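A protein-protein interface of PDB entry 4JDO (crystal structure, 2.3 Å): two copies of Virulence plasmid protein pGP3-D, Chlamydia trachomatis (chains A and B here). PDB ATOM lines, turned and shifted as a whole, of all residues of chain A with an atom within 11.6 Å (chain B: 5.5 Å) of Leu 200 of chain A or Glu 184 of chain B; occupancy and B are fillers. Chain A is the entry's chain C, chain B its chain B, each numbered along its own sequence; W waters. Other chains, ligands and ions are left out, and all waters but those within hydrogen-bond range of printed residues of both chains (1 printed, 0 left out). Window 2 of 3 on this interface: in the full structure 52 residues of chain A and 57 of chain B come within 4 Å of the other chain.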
ATOM      1  N   LYS A  83      -7.918  17.604 -18.030  1.00  0.00           N
ATOM      2  CA  LYS A  83      -7.365  18.937 -18.177  1.00  0.00           C
ATOM      3  C   LYS A  83      -6.823  19.073 -19.591  1.00  0.00           C
ATOM      4  O   LYS A  83      -5.869  18.410 -19.964  1.00  0.00           O
ATOM      5  CB  LYS A  83      -6.285  19.180 -17.134  1.00  0.00           C
ATOM      6  CG  LYS A  83      -6.752  18.903 -15.741  1.00  0.00           C
ATOM      7  CD  LYS A  83      -5.746  19.393 -14.741  1.00  0.00           C
ATOM      8  CE  LYS A  83      -4.506  18.501 -14.736  1.00  0.00           C
ATOM      9  NZ  LYS A  83      -3.509  18.960 -13.707  1.00  0.00           N
ATOM     10  N   ILE A 125     -15.431  24.930 -17.057  1.00  0.00           N
ATOM     11  CA  ILE A 125     -14.433  25.616 -16.241  1.00  0.00           C
ATOM     12  C   ILE A 125     -13.167  25.867 -17.070  1.00  0.00           C
ATOM     13  O   ILE A 125     -12.524  24.923 -17.555  1.00  0.00           O
ATOM     14  CB  ILE A 125     -14.099  24.814 -14.968  1.00  0.00           C
ATOM     15  CG1 ILE A 125     -15.382  24.464 -14.213  1.00  0.00           C
ATOM     16  CG2 ILE A 125     -13.158  25.614 -14.073  1.00  0.00           C
ATOM     17  CD1 ILE A 125     -15.181  23.507 -13.067  1.00  0.00           C
ATOM     18  N   SER A 127      -9.527  28.507 -17.873  1.00  0.00           N
ATOM     19  CA  SER A 127      -8.570  29.543 -17.477  1.00  0.00           C
ATOM     20  C   SER A 127      -7.780  30.012 -18.684  1.00  0.00           C
ATOM     21  O   SER A 127      -7.536  29.240 -19.613  1.00  0.00           O
ATOM     22  CB  SER A 127      -7.583  29.010 -16.447  1.00  0.00           C
ATOM     23  OG  SER A 127      -8.216  28.666 -15.236  1.00  0.00           O
ATOM     24  N   GLY A 155      -7.572  35.286 -15.615  1.00  0.00           N
ATOM     25  CA  GLY A 155      -6.371  34.586 -15.223  1.00  0.00           C
ATOM     26  C   GLY A 155      -6.723  33.566 -14.160  1.00  0.00           C
ATOM     27  O   GLY A 155      -6.029  32.574 -13.999  1.00  0.00           O
ATOM     28  N   VAL A 156      -7.790  33.824 -13.411  1.00  0.00           N
ATOM     29  CA  VAL A 156      -8.333  32.816 -12.511  1.00  0.00           C
ATOM     30  C   VAL A 156      -9.417  32.032 -13.250  1.00  0.00           C
ATOM     31  O   VAL A 156     -10.020  32.547 -14.204  1.00  0.00           O
ATOM     32  CB  VAL A 156      -8.905  33.433 -11.211  1.00  0.00           C
ATOM     33  CG1 VAL A 156      -7.779  34.007 -10.360  1.00  0.00           C
ATOM     34  CG2 VAL A 156      -9.942  34.496 -11.524  1.00  0.00           C
ATOM     35  N   PRO A 157      -9.642  30.772 -12.840  1.00  0.00           N
ATOM     36  CA  PRO A 157     -10.671  29.944 -13.476  1.00  0.00           C
ATOM     37  C   PRO A 157     -12.064  30.558 -13.358  1.00  0.00           C
ATOM     38  O   PRO A 157     -12.387  31.201 -12.349  1.00  0.00           O
ATOM     39  CB  PRO A 157     -10.601  28.617 -12.694  1.00  0.00           C
ATOM     40  CG  PRO A 157      -9.821  28.934 -11.432  1.00  0.00           C
ATOM     41  CD  PRO A 157      -8.875  30.023 -11.824  1.00  0.00           C
ATOM     42  N   ASN A 158     -12.870  30.343 -14.391  1.00  0.00           N
ATOM     43  CA  ASN A 158     -14.204  30.909 -14.480  1.00  0.00           C
ATOM     44  C   ASN A 158     -15.055  30.002 -15.340  1.00  0.00           C
ATOM     45  O   ASN A 158     -14.557  29.382 -16.292  1.00  0.00           O
ATOM     46  CB  ASN A 158     -14.136  32.320 -15.087  1.00  0.00           C
ATOM     47  CG  ASN A 158     -15.498  33.016 -15.138  1.00  0.00           C
ATOM     48  OD1 ASN A 158     -16.383  32.756 -14.311  1.00  0.00           O
ATOM     49  ND2 ASN A 158     -15.664  33.913 -16.106  1.00  0.00           N
ATOM     50  N   VAL A 190      -8.805  24.108 -19.874  1.00  0.00           N
ATOM     51  CA  VAL A 190     -10.080  23.623 -19.383  1.00  0.00           C
ATOM     52  C   VAL A 190      -9.865  22.724 -18.154  1.00  0.00           C
ATOM     53  O   VAL A 190      -8.996  21.841 -18.167  1.00  0.00           O
ATOM     54  CB  VAL A 190     -10.844  22.884 -20.525  1.00  0.00           C
ATOM     55  CG1 VAL A 190     -12.039  22.093 -19.984  1.00  0.00           C
ATOM     56  CG2 VAL A 190     -11.275  23.879 -21.608  1.00  0.00           C
ATOM     57  N   ASN A 191     -10.651  22.951 -17.100  1.00  0.00           N
ATOM     58  CA  ASN A 191     -10.550  22.184 -15.846  1.00  0.00           C
ATOM     59  C   ASN A 191      -9.203  22.336 -15.134  1.00  0.00           C
ATOM     60  O   ASN A 191      -8.753  21.442 -14.436  1.00  0.00           O
ATOM     61  CB  ASN A 191     -10.864  20.694 -16.058  1.00  0.00           C
ATOM     62  CG  ASN A 191     -12.322  20.446 -16.401  1.00  0.00           C
ATOM     63  OD1 ASN A 191     -13.223  21.073 -15.829  1.00  0.00           O
ATOM     64  ND2 ASN A 191     -12.563  19.529 -17.349  1.00  0.00           N
ATOM     65  N   ALA A 192      -8.572  23.486 -15.312  1.00  0.00           N
ATOM     66  CA  ALA A 192      -7.236  23.719 -14.783  1.00  0.00           C
ATOM     67  C   ALA A 192      -6.972  25.206 -14.661  1.00  0.00           C
ATOM     68  O   ALA A 192      -7.684  26.028 -15.253  1.00  0.00           O
ATOM     69  CB  ALA A 192      -6.183  23.080 -15.713  1.00  0.00           C
ATOM     70  N   LEU A 193      -5.924  25.541 -13.916  1.00  0.00           N
ATOM     71  CA  LEU A 193      -5.400  26.899 -13.861  1.00  0.00           C
ATOM     72  C   LEU A 193      -4.776  27.269 -15.207  1.00  0.00           C
ATOM     73  O   LEU A 193      -4.608  26.415 -16.087  1.00  0.00           O
ATOM     74  CB  LEU A 193      -4.373  27.008 -12.735  1.00  0.00           C
ATOM     75  CG  LEU A 193      -4.938  26.676 -11.354  1.00  0.00           C
ATOM     76  CD1 LEU A 193      -3.850  26.464 -10.304  1.00  0.00           C
ATOM     77  CD2 LEU A 193      -5.908  27.757 -10.910  1.00  0.00           C
ATOM     78  N   SER A 194      -4.415  28.538 -15.375  1.00  0.00           N
ATOM     79  CA  SER A 194      -3.892  28.990 -16.665  1.00  0.00           C
ATOM     80  C   SER A 194      -2.528  28.369 -17.013  1.00  0.00           C
ATOM     81  O   SER A 194      -2.057  28.463 -18.145  1.00  0.00           O
ATOM     82  CB  SER A 194      -3.844  30.525 -16.728  1.00  0.00           C
ATOM     83  OG  SER A 194      -2.979  31.050 -15.735  1.00  0.00           O
ATOM     84  N   ASN A 195      -1.911  27.717 -16.034  1.00  0.00           N
ATOM     85  CA  ASN A 195      -0.639  27.067 -16.246  1.00  0.00           C
ATOM     86  C   ASN A 195      -0.788  25.548 -16.411  1.00  0.00           C
ATOM     87  O   ASN A 195       0.201  24.840 -16.607  1.00  0.00           O
ATOM     88  CB  ASN A 195       0.304  27.387 -15.094  1.00  0.00           C
ATOM     89  CG  ASN A 195      -0.082  26.682 -13.816  1.00  0.00           C
ATOM     90  OD1 ASN A 195      -1.203  26.198 -13.674  1.00  0.00           O
ATOM     91  ND2 ASN A 195       0.847  26.620 -12.872  1.00  0.00           N
ATOM     92  N   GLY A 196      -2.019  25.051 -16.311  1.00  0.00           N
ATOM     93  CA  GLY A 196      -2.261  23.632 -16.479  1.00  0.00           C
ATOM     94  C   GLY A 196      -2.336  22.816 -15.206  1.00  0.00           C
ATOM     95  O   GLY A 196      -2.618  21.623 -15.263  1.00  0.00           O
ATOM     96  N   ASN A 197      -2.107  23.447 -14.061  1.00  0.00           N
ATOM     97  CA  ASN A 197      -2.239  22.771 -12.771  1.00  0.00           C
ATOM     98  C   ASN A 197      -3.690  22.648 -12.300  1.00  0.00           C
ATOM     99  O   ASN A 197      -4.562  23.341 -12.802  1.00  0.00           O
ATOM    100  CB  ASN A 197      -1.436  23.508 -11.700  1.00  0.00           C
ATOM    101  CG  ASN A 197       0.065  23.329 -11.860  1.00  0.00           C
ATOM    102  OD1 ASN A 197       0.532  22.613 -12.747  1.00  0.00           O
ATOM    103  ND2 ASN A 197       0.827  23.991 -10.997  1.00  0.00           N
ATOM    104  N   ASP A 198      -3.929  21.771 -11.328  1.00  0.00           N
ATOM    105  CA  ASP A 198      -5.256  21.601 -10.734  1.00  0.00           C
ATOM    106  C   ASP A 198      -5.745  22.839  -9.978  1.00  0.00           C
ATOM    107  O   ASP A 198      -5.008  23.438  -9.193  1.00  0.00           O
ATOM    108  CB  ASP A 198      -5.273  20.416  -9.768  1.00  0.00           C
ATOM    109  CG  ASP A 198      -5.036  19.092 -10.461  1.00  0.00           C
ATOM    110  OD1 ASP A 198      -5.292  19.004 -11.680  1.00  0.00           O
ATOM    111  OD2 ASP A 198      -4.588  18.140  -9.784  1.00  0.00           O
ATOM    112  N   ILE A 199      -7.005  23.206 -10.199  1.00  0.00           N
ATOM    113  CA  ILE A 199      -7.622  24.272  -9.414  1.00  0.00           C
ATOM    114  C   ILE A 199      -7.851  23.755  -8.013  1.00  0.00           C
ATOM    115  O   ILE A 199      -8.472  22.711  -7.827  1.00  0.00           O
ATOM    116  CB  ILE A 199      -8.959  24.711 -10.013  1.00  0.00           C
ATOM    117  CG1 ILE A 199      -8.780  25.058 -11.495  1.00  0.00           C
ATOM    118  CG2 ILE A 199      -9.525  25.871  -9.222  1.00  0.00           C
ATOM    119  CD1 ILE A 199      -9.957  24.671 -12.348  1.00  0.00           C
ATOM    120  N   LEU A 200      -7.327  24.478  -7.028  1.00  0.00           N
ATOM    121  CA  LEU A 200      -7.449  24.094  -5.619  1.00  0.00           C
ATOM    122  C   LEU A 200      -6.868  22.709  -5.340  1.00  0.00           C
ATOM    123  O   LEU A 200      -7.183  22.076  -4.332  1.00  0.00           O
ATOM    124  CB  LEU A 200      -8.903  24.220  -5.144  1.00  0.00           C
ATOM    125  CG  LEU A 200      -9.352  25.694  -5.123  1.00  0.00           C
ATOM    126  CD1 LEU A 200     -10.840  25.852  -4.816  1.00  0.00           C
ATOM    127  CD2 LEU A 200      -8.498  26.519  -4.147  1.00  0.00           C
ATOM    128  N   GLY A 201      -6.009  22.254  -6.247  1.00  0.00           N
ATOM    129  CA  GLY A 201      -5.306  20.994  -6.102  1.00  0.00           C
ATOM    130  C   GLY A 201      -6.180  19.761  -6.209  1.00  0.00           C
ATOM    131  O   GLY A 201      -5.811  18.693  -5.726  1.00  0.00           O
ATOM    132  N   ILE A 202      -7.352  19.901  -6.815  1.00  0.00           N
ATOM    133  CA  ILE A 202      -8.228  18.748  -7.006  1.00  0.00           C
ATOM    134  C   ILE A 202      -8.611  18.606  -8.467  1.00  0.00           C
ATOM    135  O   ILE A 202      -8.274  19.453  -9.286  1.00  0.00           O
ATOM    136  CB  ILE A 202      -9.502  18.816  -6.132  1.00  0.00           C
ATOM    137  CG1 ILE A 202     -10.453  19.908  -6.625  1.00  0.00           C
ATOM    138  CG2 ILE A 202      -9.143  19.050  -4.665  1.00  0.00           C
ATOM    139  CD1 ILE A 202     -11.724  19.987  -5.811  1.00  0.00           C
ATOM    140  N   THR A 203      -9.295  17.515  -8.792  1.00  0.00           N
ATOM    141  CA  THR A 203      -9.836  17.340 -10.128  1.00  0.00           C
ATOM    142  C   THR A 203     -11.183  18.052 -10.192  1.00  0.00           C
ATOM    143  O   THR A 203     -11.988  17.976  -9.260  1.00  0.00           O
ATOM    144  CB  THR A 203     -10.027  15.864 -10.461  1.00  0.00           C
ATOM    145  OG1 THR A 203     -10.680  15.231  -9.356  1.00  0.00           O
ATOM    146  CG2 THR A 203      -8.674  15.184 -10.704  1.00  0.00           C
ATOM    147  N   ASN A 204     -11.421  18.758 -11.288  1.00  0.00           N
ATOM    148  CA  ASN A 204     -12.617  19.558 -11.401  1.00  0.00           C
ATOM    149  C   ASN A 204     -13.514  19.070 -12.513  1.00  0.00           C
ATOM    150  O   ASN A 204     -13.078  18.298 -13.360  1.00  0.00           O
ATOM    151  CB  ASN A 204     -12.271  21.039 -11.538  1.00  0.00           C
ATOM    152  CG  ASN A 204     -11.989  21.669 -10.194  1.00  0.00           C
ATOM    153  OD1 ASN A 204     -12.908  21.879  -9.398  1.00  0.00           O
ATOM    154  ND2 ASN A 204     -10.710  21.919  -9.904  1.00  0.00           N
ATOM    155  N   THR A 205     -14.770  19.502 -12.503  1.00  0.00           N
ATOM    156  CA  THR A 205     -15.741  18.885 -13.395  1.00  0.00           C
ATOM    157  C   THR A 205     -16.550  19.878 -14.199  1.00  0.00           C
ATOM    158  O   THR A 205     -17.322  20.662 -13.646  1.00  0.00           O
ATOM    159  CB  THR A 205     -16.730  17.958 -12.634  1.00  0.00           C
ATOM    160  OG1 THR A 205     -16.004  16.954 -11.910  1.00  0.00           O
ATOM    161  CG2 THR A 205     -17.678  17.289 -13.614  1.00  0.00           C
ATOM    162  N   LEU B  89     -13.266  31.462   3.078  1.00  0.00           N
ATOM    163  CA  LEU B  89     -12.593  31.259   1.798  1.00  0.00           C
ATOM    164  C   LEU B  89     -12.640  29.807   1.364  1.00  0.00           C
ATOM    165  O   LEU B  89     -12.977  28.919   2.150  1.00  0.00           O
ATOM    166  CB  LEU B  89     -11.121  31.638   1.912  1.00  0.00           C
ATOM    167  CG  LEU B  89     -10.754  33.104   2.105  1.00  0.00           C
ATOM    168  CD1 LEU B  89     -11.562  33.963   1.149  1.00  0.00           C
ATOM    169  CD2 LEU B  89     -10.941  33.546   3.535  1.00  0.00           C
ATOM    170  N   PHE B  90     -12.290  29.570   0.107  1.00  0.00           N
ATOM    171  CA  PHE B  90     -11.985  28.220  -0.348  1.00  0.00           C
ATOM    172  C   PHE B  90     -10.486  28.129  -0.630  1.00  0.00           C
ATOM    173  O   PHE B  90      -9.921  28.943  -1.349  1.00  0.00           O
ATOM    174  CB  PHE B  90     -12.809  27.828  -1.580  1.00  0.00           C
ATOM    175  CG  PHE B  90     -14.240  27.434  -1.264  1.00  0.00           C
ATOM    176  CD1 PHE B  90     -14.548  26.144  -0.846  1.00  0.00           C
ATOM    177  CD2 PHE B  90     -15.273  28.350  -1.394  1.00  0.00           C
ATOM    178  CE1 PHE B  90     -15.844  25.777  -0.559  1.00  0.00           C
ATOM    179  CE2 PHE B  90     -16.584  27.983  -1.106  1.00  0.00           C
ATOM    180  CZ  PHE B  90     -16.863  26.700  -0.691  1.00  0.00           C
ATOM    181  N   THR B  91      -9.846  27.139  -0.034  1.00  0.00           N
ATOM    182  CA  THR B  91      -8.409  26.968  -0.156  1.00  0.00           C
ATOM    183  C   THR B  91      -8.147  25.508  -0.527  1.00  0.00           C
ATOM    184  O   THR B  91      -9.049  24.664  -0.389  1.00  0.00           O
ATOM    185  CB  THR B  91      -7.738  27.275   1.186  1.00  0.00           C
ATOM    186  OG1 THR B  91      -8.220  26.351   2.170  1.00  0.00           O
ATOM    187  CG2 THR B  91      -8.071  28.697   1.635  1.00  0.00           C
ATOM    188  N   PRO B  92      -6.920  25.194  -0.999  1.00  0.00           N
ATOM    189  CA  PRO B  92      -6.629  23.783  -1.276  1.00  0.00           C
ATOM    190  C   PRO B  92      -6.850  22.943  -0.021  1.00  0.00           C
ATOM    191  O   PRO B  92      -7.226  21.773  -0.114  1.00  0.00           O
ATOM    192  CB  PRO B  92      -5.147  23.800  -1.657  1.00  0.00           C
ATOM    193  CG  PRO B  92      -4.912  25.172  -2.169  1.00  0.00           C
ATOM    194  CD  PRO B  92      -5.775  26.062  -1.326  1.00  0.00           C
ATOM    195  N   ILE B  95     -11.100  22.792   0.551  1.00  0.00           N
ATOM    196  CA  ILE B  95     -11.979  22.468  -0.573  1.00  0.00           C
ATOM    197  C   ILE B  95     -12.622  21.074  -0.513  1.00  0.00           C
ATOM    198  O   ILE B  95     -13.701  20.856  -1.071  1.00  0.00           O
ATOM    199  CB  ILE B  95     -11.277  22.680  -1.933  1.00  0.00           C
ATOM    200  CG1 ILE B  95     -12.298  22.559  -3.062  1.00  0.00           C
ATOM    201  CG2 ILE B  95     -10.107  21.721  -2.107  1.00  0.00           C
ATOM    202  CD1 ILE B  95     -13.546  23.403  -2.843  1.00  0.00           C
ATOM    203  N   VAL B 134     -15.871  30.949  -5.667  1.00  0.00           N
ATOM    204  CA  VAL B 134     -16.022  29.498  -5.669  1.00  0.00           C
ATOM    205  C   VAL B 134     -17.399  29.105  -5.127  1.00  0.00           C
ATOM    206  O   VAL B 134     -17.860  29.633  -4.110  1.00  0.00           O
ATOM    207  CB  VAL B 134     -14.911  28.801  -4.849  1.00  0.00           C
ATOM    208  CG1 VAL B 134     -15.167  27.289  -4.759  1.00  0.00           C
ATOM    209  CG2 VAL B 134     -13.531  29.068  -5.464  1.00  0.00           C
ATOM    210  N   TYR B 150     -17.001  27.759 -10.451  1.00  0.00           N
ATOM    211  CA  TYR B 150     -16.199  28.976 -10.324  1.00  0.00           C
ATOM    212  C   TYR B 150     -16.842  30.135 -11.039  1.00  0.00           C
ATOM    213  O   TYR B 150     -17.434  29.975 -12.111  1.00  0.00           O
ATOM    214  CB  TYR B 150     -14.775  28.768 -10.854  1.00  0.00           C
ATOM    215  CG  TYR B 150     -14.103  27.621 -10.166  1.00  0.00           C
ATOM    216  CD1 TYR B 150     -14.252  26.320 -10.638  1.00  0.00           C
ATOM    217  CD2 TYR B 150     -13.382  27.818  -8.997  1.00  0.00           C
ATOM    218  CE1 TYR B 150     -13.655  25.252  -9.981  1.00  0.00           C
ATOM    219  CE2 TYR B 150     -12.788  26.764  -8.339  1.00  0.00           C
ATOM    220  CZ  TYR B 150     -12.926  25.485  -8.838  1.00  0.00           C
ATOM    221  OH  TYR B 150     -12.353  24.432  -8.176  1.00  0.00           O
ATOM    222  N   GLY B 182     -14.530  33.376  -1.534  1.00  0.00           N
ATOM    223  CA  GLY B 182     -13.451  33.765  -2.423  1.00  0.00           C
ATOM    224  C   GLY B 182     -12.507  32.619  -2.732  1.00  0.00           C
ATOM    225  O   GLY B 182     -12.326  31.686  -1.932  1.00  0.00           O
ATOM    226  N   LEU B 183     -11.917  32.668  -3.918  1.00  0.00           N
ATOM    227  CA  LEU B 183     -10.887  31.708  -4.289  1.00  0.00           C
ATOM    228  C   LEU B 183      -9.572  32.099  -3.591  1.00  0.00           C
ATOM    229  O   LEU B 183      -8.938  33.091  -3.947  1.00  0.00           O
ATOM    230  CB  LEU B 183     -10.729  31.661  -5.812  1.00  0.00           C
ATOM    231  CG  LEU B 183      -9.545  30.904  -6.431  1.00  0.00           C
ATOM    232  CD1 LEU B 183      -9.720  29.393  -6.325  1.00  0.00           C
ATOM    233  CD2 LEU B 183      -9.373  31.313  -7.880  1.00  0.00           C
ATOM    234  N   GLU B 184      -9.212  31.338  -2.559  1.00  0.00           N
ATOM    235  CA  GLU B 184      -7.987  31.551  -1.788  1.00  0.00           C
ATOM    236  C   GLU B 184      -7.821  32.881  -1.013  1.00  0.00           C
ATOM    237  O   GLU B 184      -7.150  32.912   0.005  1.00  0.00           O
ATOM    238  CB  GLU B 184      -6.773  31.235  -2.648  1.00  0.00           C
ATOM    239  CG  GLU B 184      -6.727  29.764  -2.984  1.00  0.00           C
ATOM    240  CD  GLU B 184      -5.675  29.426  -4.004  1.00  0.00           C
ATOM    241  OE1 GLU B 184      -5.463  30.252  -4.924  1.00  0.00           O
ATOM    242  OE2 GLU B 184      -5.058  28.337  -3.884  1.00  0.00           O
ATOM    243  N   SER B 185      -8.439  33.964  -1.471  1.00  0.00           N
ATOM    244  CA  SER B 185      -8.457  35.208  -0.700  1.00  0.00           C
ATOM    245  C   SER B 185      -9.685  36.044  -1.042  1.00  0.00           C
ATOM    246  O   SER B 185     -10.405  35.741  -1.997  1.00  0.00           O
ATOM    247  CB  SER B 185      -7.204  36.028  -0.985  1.00  0.00           C
ATOM    248  OG  SER B 185      -7.171  36.373  -2.358  1.00  0.00           O
ATOM    249  N   GLY B 186      -9.913  37.097  -0.262  1.00  0.00           N
ATOM    250  CA  GLY B 186     -10.925  38.095  -0.583  1.00  0.00           C
ATOM    251  C   GLY B 186     -12.292  37.859   0.036  1.00  0.00           C
ATOM    252  O   GLY B 186     -12.641  36.740   0.393  1.00  0.00           O
HETATM  253  O   HOH W   1      -6.888  20.039  -2.237  1.00  0.00           O
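The side-chain hydroxyl of Tyr 150 of chain B lies within hydrogen-bond range of the side-chain amide oxygen of Asn 204 of chain A (2.9 Å).
The backbone carbonyl oxygen (O) of Ile 199 of chain A lies within hydrogen-bond range of the side-chain amide nitrogen (ND2) of Asn 204 of chain A. The backbone carbonyl oxygen of Phe 90 of chain B lies within hydrogen-bond range of the backbone NH of Glu 184 of chain B (2.8 Å). The backbone carbonyl oxygen (O) of Ile 125 of chain A lies within hydrogen-bond range of the backbone NH (N) of Asn 191 of chain A. The backbone carbonyl oxygen (O) of Gly 182 of chain B lies within hydrogen-bond range of the backbone NH (N) of Phe 90 of chain B, at 2.9 Å.
Among the printed residues, pairs that only touch across the chains: Ile 199 of chain A with Tyr 150 of chain B (3.3 Å), Leu 200 of chain A with Pro 92 of chain B (3.5 Å), Ile 125 of chain A with Tyr 150 of chain B (3.7 Å), Leu 200 of chain A with Ile 95 of chain B (3.7 Å), Asn 158 of chain A with Tyr 150 of chain B (3.7 Å), Pro 157 of chain A with Tyr 150 of chain B (3.7 Å), Leu 200 of chain A with Thr 91 of chain B (3.8 Å), Leu 200 of chain A with Leu 183 of chain B (3.8 Å), Ile 202 of chain A with Ile 95 of chain B (3.8 Å), Leu 200 of chain A with Glu 184 of chain B (3.9 Å), Leu 200 of chain A with Tyr 150 of chain B (3.9 Å), Leu 200 of chain A with Phe 90 of chain B (3.97 Å) and Val 156 of chain A with Leu 183 of chain B (3.98 Å).
Leu 200 of chain A touches seven residues of chain B. Glu 184 of chain B touches just one residue of chain A: Leu 200 (3.9 Å). Leu 89 of chain B touches none of the printed residues of chain A. Of the printed residues of chain A, Phe 90 of chain B touches Leu 200. Pro 92 of chain B touches one residue of chain A. Of chain A, only Leu 200 and Ile 202 come within 4 Å of Ile 95 of chain B. No residue of chain A comes within 4 Å of Gly 182 of chain B. No residue of chain A comes within 4 Å of Gly 186 of chain B. Printed residues of chain B within 4 Å of Ile 202 of chain A: Ile 95 (3.8 Å). Of the printed residues of chain B, Pro 157 of chain A touches Tyr 150. Printed residues of chain B within 4 Å of Asn 158 of chain A: Tyr 150 (3.7 Å). Of the printed residues of chain B, Val 156 of chain A touches Leu 183. Of the printed residues of chain B, Asn 204 of chain A touches Tyr 150. Ala 192 of chain A touches none of the printed residues of chain B.
Printed residues of chain A that touch a printed residue of chain B: Ile 125, Val 156, Pro 157, Asn 158, Ile 199, Leu 200, Ile 202 and Asn 204. Of the 12 printed residues of chain B, 7 touch a printed residue of chain A. Among the printed residues, 14 pairs touch across the chains. Among the printed residues, no Asp or Glu carboxylate lies within 4 Å of a Lys or Arg side-chain nitrogen of the other chain.
No position is printed for both chains.
Water W1 bridges O of Pro 92 of chain B (2.8 Å) and O of Leu 200 of chain A (2.9 Å).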
